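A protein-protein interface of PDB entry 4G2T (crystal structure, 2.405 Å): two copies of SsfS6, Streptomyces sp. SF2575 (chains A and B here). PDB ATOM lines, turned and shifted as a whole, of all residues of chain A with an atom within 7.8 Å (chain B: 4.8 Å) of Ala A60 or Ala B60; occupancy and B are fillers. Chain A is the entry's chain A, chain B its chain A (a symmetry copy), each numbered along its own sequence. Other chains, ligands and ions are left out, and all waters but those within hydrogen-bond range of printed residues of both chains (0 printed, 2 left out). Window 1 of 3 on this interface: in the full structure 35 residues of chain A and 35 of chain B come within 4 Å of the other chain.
Of the 10 printed residues of chain B, 7 touch a printed residue of chain A.
Printed residues of chain B that touch a printed residue of chain A: Val B32, Trp B36, Thr B58, Gly B59, Ala B60, Gly B61 and Tyr B209.
Of the 20 printed residues of chain A, 8 touch a printed residue of chain B.
Printed residues of chain A that touch a printed residue of chain B: Val A32, Trp A36, Thr A58, Gly A59, Ala A60, Gly A61, Tyr A209 and Arg A212.
Among the printed residues, 15 pairs touch across the chains.
Among the printed residues, no Asp or Glu carboxylate lies within 4 Å of a Lys or Arg side-chain nitrogen of the other chain.
The backbone carbonyl oxygen of Gly A59 lies close to the backbone carbonyl oxygen of Thr B58, 3.1 Å away.
The side-chain hydroxyl (OG1) of Thr B58 lies within hydrogen-bond range of the guanidinium group (NH2) of Arg A212 (3.0 Å).
O of Ala B60 lies close to O of Ala A60 (3.1 Å).
The backbone carbonyl oxygen (O) of Thr A58 sits close to the backbone carbonyl oxygen (O) of Gly B59 (3.1 Å).
The backbone NH of Gly A61 sits at hydrogen-bond distance from the backbone carbonyl oxygen of Gly B59.
The indole nitrogen of Trp B36 lies close to the indole nitrogen of Trp A36, 3.4 Å away.
The guanidinium group of Arg A212 lies close to the backbone NH of Gly B59, at 3.4 Å.
The backbone NH (N) of Gly B61 is in hydrogen-bond range of the backbone carbonyl oxygen (O) of Gly A59 (3.4 Å).
Val A32 touches Trp B36, and with the chains exchanged Trp A36 touches Val B32.
Trp A36 touches its own counterpart, Trp B36.
Ala B60 touches its own counterpart, Ala A60.
Ala A60 touches Gly B61, and with the chains exchanged Gly A61 touches Ala B60.
Positions printed for both chains: 32, 36, 56, 57, 58, 59, 60, 61, 62 and 209.
Of the 15 pairs that touch across the chains among the printed residues, 13 have their exchanged pair printed and touching as well.
Trp B36 touches Val A32 (CH2 to CG1, 3.9 Å).
Trp A36 touches Val B32.
Gly A59 touches Gly B59.
Ala A60 touches Gly B61.
O of Ala B60 touches CA of Gly A61, at 3.8 Å.
Gly A61 touches Tyr B209 (O to CE1, 3.6 Å).
Tyr A209 touches Gly B61 (CE1 to O, 3.6 Å).
Printed residues of chain B within 4 Å of Ala A60: Ala B60 and Gly B61.
Leu A62 touches none of the printed residues of chain B.
Printed residues of chain A within 4 Å of Trp B36: Val A32 (3.9 Å) and Trp A36 (3.4 Å).
Gly B59 touches just these residues of chain A: Thr A58, Gly A59, Gly A61 and Arg A212.
Of the printed residues of chain A, Ala B60 touches Ala A60 (3.1 Å) and Gly A61 (3.8 Å).
Of the printed residues of chain A, Gly B61 touches Gly A59, Ala A60 and Tyr A209.
The nearest printed residue of chain B that does not touch Ala A60 is Trp B36 (4.002 Å).
The nearest printed residue of chain B that does not touch Gly A59 is Ala B60 (4.3 Å).
O of Gly B59 sits at hydrogen-bond distance from OH of Tyr B209 (3.3 Å).
The backbone carbonyl oxygen (O) of Ala A60 lies within hydrogen-bond range of the indole nitrogen (NE1) of Trp A36, at 2.7 Å.
OH of Tyr A209 lies within hydrogen-bond range of O of Gly A211 (3.4 Å).
O of Gly A59 sits at hydrogen-bond distance from OH of Tyr A209, 3.3 Å away.
O of Gly A54 is in hydrogen-bond range of OG1 of Thr A58 (3.2 Å).
The backbone carbonyl oxygen (O) of Ala B60 is in hydrogen-bond range of the indole nitrogen (NE1) of Trp B36 (2.7 Å).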
ATOM      1  N   VAL A  28       4.525  28.393 -31.832  1.00  0.00           N
ATOM      2  CA  VAL A  28       4.992  27.100 -31.341  1.00  0.00           C
ATOM      3  C   VAL A  28       4.400  25.939 -32.134  1.00  0.00           C
ATOM      4  O   VAL A  28       5.127  25.074 -32.621  1.00  0.00           O
ATOM      5  CB  VAL A  28       4.657  26.909 -29.851  1.00  0.00           C
ATOM      6  CG1 VAL A  28       5.108  25.533 -29.378  1.00  0.00           C
ATOM      7  CG2 VAL A  28       5.303  28.003 -29.017  1.00  0.00           C
ATOM      8  N   MET A  29       3.076  25.933 -32.252  1.00  0.00           N
ATOM      9  CA  MET A  29       2.347  24.871 -32.950  1.00  0.00           C
ATOM     10  C   MET A  29       2.835  24.516 -34.367  1.00  0.00           C
ATOM     11  O   MET A  29       2.933  23.336 -34.699  1.00  0.00           O
ATOM     12  CB  MET A  29       0.844  25.170 -32.963  1.00  0.00           C
ATOM     13  CG  MET A  29       0.212  25.208 -31.582  1.00  0.00           C
ATOM     14  SD  MET A  29      -1.670  25.714 -31.626  1.00  0.00           S
ATOM     15  CE  MET A  29      -2.076  25.505 -29.730  1.00  0.00           C
ATOM     16  N   LEU A  31       5.677  24.465 -35.506  1.00  0.00           N
ATOM     17  CA  LEU A  31       6.978  23.804 -35.457  1.00  0.00           C
ATOM     18  C   LEU A  31       6.849  22.354 -34.997  1.00  0.00           C
ATOM     19  O   LEU A  31       7.796  21.574 -35.097  1.00  0.00           O
ATOM     20  CB  LEU A  31       7.940  24.559 -34.537  1.00  0.00           C
ATOM     21  CG  LEU A  31       8.527  25.865 -35.074  1.00  0.00           C
ATOM     22  CD1 LEU A  31       9.463  26.490 -34.052  1.00  0.00           C
ATOM     23  CD2 LEU A  31       9.251  25.622 -36.389  1.00  0.00           C
ATOM     24  N   VAL A  32       5.672  22.006 -34.490  1.00  0.00           N
ATOM     25  CA  VAL A  32       5.401  20.652 -34.001  1.00  0.00           C
ATOM     26  C   VAL A  32       5.524  19.529 -35.049  1.00  0.00           C
ATOM     27  O   VAL A  32       6.165  18.513 -34.776  1.00  0.00           O
ATOM     28  CB  VAL A  32       4.029  20.570 -33.279  1.00  0.00           C
ATOM     29  CG1 VAL A  32       3.658  19.123 -32.984  1.00  0.00           C
ATOM     30  CG2 VAL A  32       4.053  21.393 -32.002  1.00  0.00           C
ATOM     31  N   PRO A  33       4.917  19.697 -36.243  1.00  0.00           N
ATOM     32  CA  PRO A  33       4.991  18.603 -37.222  1.00  0.00           C
ATOM     33  C   PRO A  33       6.416  18.253 -37.650  1.00  0.00           C
ATOM     34  O   PRO A  33       6.739  17.071 -37.765  1.00  0.00           O
ATOM     35  CB  PRO A  33       4.211  19.155 -38.419  1.00  0.00           C
ATOM     36  CG  PRO A  33       3.290  20.154 -37.833  1.00  0.00           C
ATOM     37  CD  PRO A  33       4.067  20.797 -36.735  1.00  0.00           C
ATOM     38  N   TRP A  36       8.237  16.461 -34.763  1.00  0.00           N
ATOM     39  CA  TRP A  36       7.849  15.057 -34.691  1.00  0.00           C
ATOM     40  C   TRP A  36       8.372  14.275 -35.889  1.00  0.00           C
ATOM     41  O   TRP A  36       8.637  13.079 -35.789  1.00  0.00           O
ATOM     42  CB  TRP A  36       6.331  14.910 -34.581  1.00  0.00           C
ATOM     43  CG  TRP A  36       5.863  14.677 -33.179  1.00  0.00           C
ATOM     44  CD1 TRP A  36       5.124  15.526 -32.408  1.00  0.00           C
ATOM     45  CD2 TRP A  36       6.119  13.519 -32.373  1.00  0.00           C
ATOM     46  NE1 TRP A  36       4.895  14.965 -31.174  1.00  0.00           N
ATOM     47  CE2 TRP A  36       5.495  13.735 -31.127  1.00  0.00           C
ATOM     48  CE3 TRP A  36       6.809  12.323 -32.585  1.00  0.00           C
ATOM     49  CZ2 TRP A  36       5.543  12.796 -30.098  1.00  0.00           C
ATOM     50  CZ3 TRP A  36       6.855  11.392 -31.560  1.00  0.00           C
ATOM     51  CH2 TRP A  36       6.226  11.634 -30.333  1.00  0.00           C
ATOM     52  N   VAL A  47      12.247  20.926 -27.313  1.00  0.00           N
ATOM     53  CA  VAL A  47      11.669  22.225 -27.627  1.00  0.00           C
ATOM     54  C   VAL A  47      11.895  23.221 -26.496  1.00  0.00           C
ATOM     55  O   VAL A  47      11.451  23.011 -25.367  1.00  0.00           O
ATOM     56  CB  VAL A  47      10.166  22.124 -27.925  1.00  0.00           C
ATOM     57  CG1 VAL A  47       9.626  23.475 -28.367  1.00  0.00           C
ATOM     58  CG2 VAL A  47       9.906  21.068 -28.988  1.00  0.00           C
ATOM     59  N   GLY A  54       4.942  25.831 -22.136  1.00  0.00           N
ATOM     60  CA  GLY A  54       5.152  24.464 -21.690  1.00  0.00           C
ATOM     61  C   GLY A  54       4.027  23.501 -22.031  1.00  0.00           C
ATOM     62  O   GLY A  54       4.252  22.520 -22.740  1.00  0.00           O
ATOM     63  N   PRO A  55       2.812  23.764 -21.517  1.00  0.00           N
ATOM     64  CA  PRO A  55       1.642  22.921 -21.791  1.00  0.00           C
ATOM     65  C   PRO A  55       1.349  22.746 -23.282  1.00  0.00           C
ATOM     66  O   PRO A  55       0.832  21.703 -23.680  1.00  0.00           O
ATOM     67  CB  PRO A  55       0.501  23.689 -21.120  1.00  0.00           C
ATOM     68  CG  PRO A  55       1.158  24.409 -20.000  1.00  0.00           C
ATOM     69  CD  PRO A  55       2.509  24.808 -20.518  1.00  0.00           C
ATOM     70  N   THR A  56       1.673  23.752 -24.089  1.00  0.00           N
ATOM     71  CA  THR A  56       1.469  23.669 -25.531  1.00  0.00           C
ATOM     72  C   THR A  56       2.442  22.675 -26.161  1.00  0.00           C
ATOM     73  O   THR A  56       2.048  21.827 -26.963  1.00  0.00           O
ATOM     74  CB  THR A  56       1.637  25.044 -26.209  1.00  0.00           C
ATOM     75  OG1 THR A  56       0.677  25.964 -25.674  1.00  0.00           O
ATOM     76  CG2 THR A  56       1.436  24.929 -27.712  1.00  0.00           C
ATOM     77  N   VAL A  57       3.712  22.785 -25.787  1.00  0.00           N
ATOM     78  CA  VAL A  57       4.753  21.900 -26.299  1.00  0.00           C
ATOM     79  C   VAL A  57       4.527  20.454 -25.875  1.00  0.00           C
ATOM     80  O   VAL A  57       4.525  19.542 -26.703  1.00  0.00           O
ATOM     81  CB  VAL A  57       6.145  22.341 -25.809  1.00  0.00           C
ATOM     82  CG1 VAL A  57       7.184  21.278 -26.129  1.00  0.00           C
ATOM     83  CG2 VAL A  57       6.525  23.682 -26.421  1.00  0.00           C
ATOM     84  N   THR A  58       4.336  20.253 -24.577  1.00  0.00           N
ATOM     85  CA  THR A  58       4.172  18.915 -24.025  1.00  0.00           C
ATOM     86  C   THR A  58       2.813  18.326 -24.389  1.00  0.00           C
ATOM     87  O   THR A  58       2.649  17.107 -24.443  1.00  0.00           O
ATOM     88  CB  THR A  58       4.343  18.925 -22.502  1.00  0.00           C
ATOM     89  OG1 THR A  58       3.240  19.610 -21.899  1.00  0.00           O
ATOM     90  CG2 THR A  58       5.633  19.634 -22.131  1.00  0.00           C
ATOM     91  N   GLY A  59       1.844  19.199 -24.646  1.00  0.00           N
ATOM     92  CA  GLY A  59       0.536  18.769 -25.104  1.00  0.00           C
ATOM     93  C   GLY A  59       0.600  18.237 -26.523  1.00  0.00           C
ATOM     94  O   GLY A  59      -0.332  17.589 -26.998  1.00  0.00           O
ATOM     95  N   ALA A  60       1.708  18.518 -27.200  1.00  0.00           N
ATOM     96  CA  ALA A  60       1.946  18.011 -28.545  1.00  0.00           C
ATOM     97  C   ALA A  60       2.799  16.747 -28.501  1.00  0.00           C
ATOM     98  O   ALA A  60       3.136  16.178 -29.540  1.00  0.00           O
ATOM     99  CB  ALA A  60       2.612  19.075 -29.402  1.00  0.00           C
ATOM    100  N   GLY A  61       3.150  16.316 -27.292  1.00  0.00           N
ATOM    101  CA  GLY A  61       3.921  15.101 -27.106  1.00  0.00           C
ATOM    102  C   GLY A  61       5.422  15.306 -27.196  1.00  0.00           C
ATOM    103  O   GLY A  61       6.175  14.350 -27.381  1.00  0.00           O
ATOM    104  N   LEU A  62       5.860  16.553 -27.055  1.00  0.00           N
ATOM    105  CA  LEU A  62       7.274  16.888 -27.191  1.00  0.00           C
ATOM    106  C   LEU A  62       7.903  17.287 -25.858  1.00  0.00           C
ATOM    107  O   LEU A  62       7.240  17.882 -25.009  1.00  0.00           O
ATOM    108  CB  LEU A  62       7.452  18.017 -28.210  1.00  0.00           C
ATOM    109  CG  LEU A  62       7.038  17.693 -29.646  1.00  0.00           C
ATOM    110  CD1 LEU A  62       7.127  18.933 -30.522  1.00  0.00           C
ATOM    111  CD2 LEU A  62       7.898  16.572 -30.209  1.00  0.00           C
ATOM    112  N   PRO A  63       9.189  16.949 -25.671  1.00  0.00           N
ATOM    113  CA  PRO A  63       9.948  17.352 -24.480  1.00  0.00           C
ATOM    114  C   PRO A  63      10.093  18.869 -24.415  1.00  0.00           C
ATOM    115  O   PRO A  63      10.254  19.508 -25.454  1.00  0.00           O
ATOM    116  CB  PRO A  63      11.320  16.706 -24.704  1.00  0.00           C
ATOM    117  CG  PRO A  63      11.064  15.581 -25.647  1.00  0.00           C
ATOM    118  CD  PRO A  63       9.974  16.065 -26.549  1.00  0.00           C
ATOM    119  N   TYR A 209      -0.940  21.542 -37.219  1.00  0.00           N
ATOM    120  CA  TYR A 209      -1.176  21.152 -35.834  1.00  0.00           C
ATOM    121  C   TYR A 209      -1.799  22.331 -35.095  1.00  0.00           C
ATOM    122  O   TYR A 209      -1.218  23.415 -35.041  1.00  0.00           O
ATOM    123  CB  TYR A 209       0.114  20.712 -35.140  1.00  0.00           C
ATOM    124  CG  TYR A 209      -0.100  20.373 -33.682  1.00  0.00           C
ATOM    125  CD1 TYR A 209      -0.735  19.194 -33.312  1.00  0.00           C
ATOM    126  CD2 TYR A 209       0.315  21.236 -32.676  1.00  0.00           C
ATOM    127  CE1 TYR A 209      -0.944  18.881 -31.983  1.00  0.00           C
ATOM    128  CE2 TYR A 209       0.111  20.931 -31.343  1.00  0.00           C
ATOM    129  CZ  TYR A 209      -0.518  19.752 -31.004  1.00  0.00           C
ATOM    130  OH  TYR A 209      -0.726  19.443 -29.679  1.00  0.00           O
ATOM    131  N   GLY A 211      -3.242  22.276 -31.775  1.00  0.00           N
ATOM    132  CA  GLY A 211      -3.371  22.161 -30.335  1.00  0.00           C
ATOM    133  C   GLY A 211      -3.958  20.853 -29.844  1.00  0.00           C
ATOM    134  O   GLY A 211      -3.994  19.858 -30.567  1.00  0.00           O
ATOM    135  N   ARG A 212      -4.435  20.873 -28.604  1.00  0.00           N
ATOM    136  CA  ARG A 212      -4.846  19.662 -27.905  1.00  0.00           C
ATOM    137  C   ARG A 212      -6.280  19.754 -27.392  1.00  0.00           C
ATOM    138  O   ARG A 212      -6.634  20.695 -26.682  1.00  0.00           O
ATOM    139  CB  ARG A 212      -3.895  19.411 -26.734  1.00  0.00           C
ATOM    140  CG  ARG A 212      -4.181  18.162 -25.923  1.00  0.00           C
ATOM    141  CD  ARG A 212      -3.553  18.283 -24.544  1.00  0.00           C
ATOM    142  NE  ARG A 212      -3.408  16.995 -23.875  1.00  0.00           N
ATOM    143  CZ  ARG A 212      -4.375  16.392 -23.192  1.00  0.00           C
ATOM    144  NH1 ARG A 212      -5.573  16.954 -23.096  1.00  0.00           N
ATOM    145  NH2 ARG A 212      -4.147  15.221 -22.612  1.00  0.00           N
ATOM    146  N   VAL B  32       2.381   5.689 -30.683  1.00  0.00           N
ATOM    147  CA  VAL B  32       2.516   7.125 -30.935  1.00  0.00           C
ATOM    148  C   VAL B  32       3.585   7.522 -31.972  1.00  0.00           C
ATOM    149  O   VAL B  32       3.297   8.323 -32.863  1.00  0.00           O
ATOM    150  CB  VAL B  32       2.722   7.919 -29.616  1.00  0.00           C
ATOM    151  CG1 VAL B  32       3.092   9.367 -29.908  1.00  0.00           C
ATOM    152  CG2 VAL B  32       1.474   7.842 -28.752  1.00  0.00           C
ATOM    153  N   TRP B  36       2.714   9.467 -35.481  1.00  0.00           N
ATOM    154  CA  TRP B  36       3.256  10.776 -35.824  1.00  0.00           C
ATOM    155  C   TRP B  36       4.129  10.706 -37.069  1.00  0.00           C
ATOM    156  O   TRP B  36       4.234  11.677 -37.816  1.00  0.00           O
ATOM    157  CB  TRP B  36       4.043  11.368 -34.654  1.00  0.00           C
ATOM    158  CG  TRP B  36       3.257  12.367 -33.862  1.00  0.00           C
ATOM    159  CD1 TRP B  36       2.822  12.235 -32.577  1.00  0.00           C
ATOM    160  CD2 TRP B  36       2.800  13.648 -34.314  1.00  0.00           C
ATOM    161  NE1 TRP B  36       2.128  13.358 -32.195  1.00  0.00           N
ATOM    162  CE2 TRP B  36       2.099  14.240 -33.243  1.00  0.00           C
ATOM    163  CE3 TRP B  36       2.917  14.352 -35.516  1.00  0.00           C
ATOM    164  CZ2 TRP B  36       1.519  15.503 -33.341  1.00  0.00           C
ATOM    165  CZ3 TRP B  36       2.339  15.608 -35.610  1.00  0.00           C
ATOM    166  CH2 TRP B  36       1.649  16.169 -34.529  1.00  0.00           C
ATOM    167  N   THR B  56      -4.112  10.344 -22.721  1.00  0.00           N
ATOM    168  CA  THR B  56      -2.839   9.775 -23.150  1.00  0.00           C
ATOM    169  C   THR B  56      -2.603  10.030 -24.636  1.00  0.00           C
ATOM    170  O   THR B  56      -1.520  10.459 -25.040  1.00  0.00           O
ATOM    171  CB  THR B  56      -2.775   8.258 -22.879  1.00  0.00           C
ATOM    172  OG1 THR B  56      -2.923   8.014 -21.474  1.00  0.00           O
ATOM    173  CG2 THR B  56      -1.447   7.684 -23.348  1.00  0.00           C
ATOM    174  N   VAL B  57      -3.625   9.770 -25.443  1.00  0.00           N
ATOM    175  CA  VAL B  57      -3.550   9.973 -26.885  1.00  0.00           C
ATOM    176  C   VAL B  57      -3.363  11.443 -27.242  1.00  0.00           C
ATOM    177  O   VAL B  57      -2.457  11.804 -27.995  1.00  0.00           O
ATOM    178  CB  VAL B  57      -4.822   9.459 -27.585  1.00  0.00           C
ATOM    179  CG1 VAL B  57      -4.847   9.905 -29.039  1.00  0.00           C
ATOM    180  CG2 VAL B  57      -4.917   7.944 -27.473  1.00  0.00           C
ATOM    181  N   THR B  58      -4.227  12.288 -26.693  1.00  0.00           N
ATOM    182  CA  THR B  58      -4.204  13.712 -26.997  1.00  0.00           C
ATOM    183  C   THR B  58      -3.009  14.401 -26.347  1.00  0.00           C
ATOM    184  O   THR B  58      -2.541  15.434 -26.825  1.00  0.00           O
ATOM    185  CB  THR B  58      -5.503  14.390 -26.547  1.00  0.00           C
ATOM    186  OG1 THR B  58      -5.562  14.413 -25.116  1.00  0.00           O
ATOM    187  CG2 THR B  58      -6.699  13.624 -27.082  1.00  0.00           C
ATOM    188  N   GLY B  59      -2.514  13.818 -25.261  1.00  0.00           N
ATOM    189  CA  GLY B  59      -1.317  14.315 -24.609  1.00  0.00           C
ATOM    190  C   GLY B  59      -0.085  14.056 -25.457  1.00  0.00           C
ATOM    191  O   GLY B  59       0.981  14.624 -25.215  1.00  0.00           O
ATOM    192  N   ALA B  60      -0.236  13.192 -26.454  1.00  0.00           N
ATOM    193  CA  ALA B  60       0.834  12.901 -27.399  1.00  0.00           C
ATOM    194  C   ALA B  60       0.679  13.740 -28.664  1.00  0.00           C
ATOM    195  O   ALA B  60       1.470  13.620 -29.600  1.00  0.00           O
ATOM    196  CB  ALA B  60       0.851  11.420 -27.739  1.00  0.00           C
ATOM    197  N   GLY B  61      -0.349  14.583 -28.688  1.00  0.00           N
ATOM    198  CA  GLY B  61      -0.586  15.472 -29.810  1.00  0.00           C
ATOM    199  C   GLY B  61      -1.396  14.845 -30.931  1.00  0.00           C
ATOM    200  O   GLY B  61      -1.400  15.344 -32.056  1.00  0.00           O
ATOM    201  N   LEU B  62      -2.090  13.755 -30.622  1.00  0.00           N
ATOM    202  CA  LEU B  62      -2.851  13.021 -31.629  1.00  0.00           C
ATOM    203  C   LEU B  62      -4.358  13.158 -31.425  1.00  0.00           C
ATOM    204  O   LEU B  62      -4.828  13.254 -30.291  1.00  0.00           O
ATOM    205  CB  LEU B  62      -2.455  11.543 -31.614  1.00  0.00           C
ATOM    206  CG  LEU B  62      -1.006  11.234 -31.990  1.00  0.00           C
ATOM    207  CD1 LEU B  62      -0.705   9.756 -31.798  1.00  0.00           C
ATOM    208  CD2 LEU B  62      -0.726  11.659 -33.424  1.00  0.00           C
ATOM    209  N   TYR B 209       8.293   6.580 -26.728  1.00  0.00           N
ATOM    210  CA  TYR B 209       7.436   7.636 -26.202  1.00  0.00           C
ATOM    211  C   TYR B 209       6.871   7.182 -24.861  1.00  0.00           C
ATOM    212  O   TYR B 209       6.211   6.146 -24.777  1.00  0.00           O
ATOM    213  CB  TYR B 209       6.302   7.981 -27.168  1.00  0.00           C
ATOM    214  CG  TYR B 209       5.362   9.025 -26.606  1.00  0.00           C
ATOM    215  CD1 TYR B 209       5.743  10.358 -26.532  1.00  0.00           C
ATOM    216  CD2 TYR B 209       4.102   8.676 -26.134  1.00  0.00           C
ATOM    217  CE1 TYR B 209       4.894  11.316 -26.010  1.00  0.00           C
ATOM    218  CE2 TYR B 209       3.247   9.628 -25.613  1.00  0.00           C
ATOM    219  CZ  TYR B 209       3.648  10.946 -25.554  1.00  0.00           C
ATOM    220  OH  TYR B 209       2.803  11.898 -25.034  1.00  0.00           O
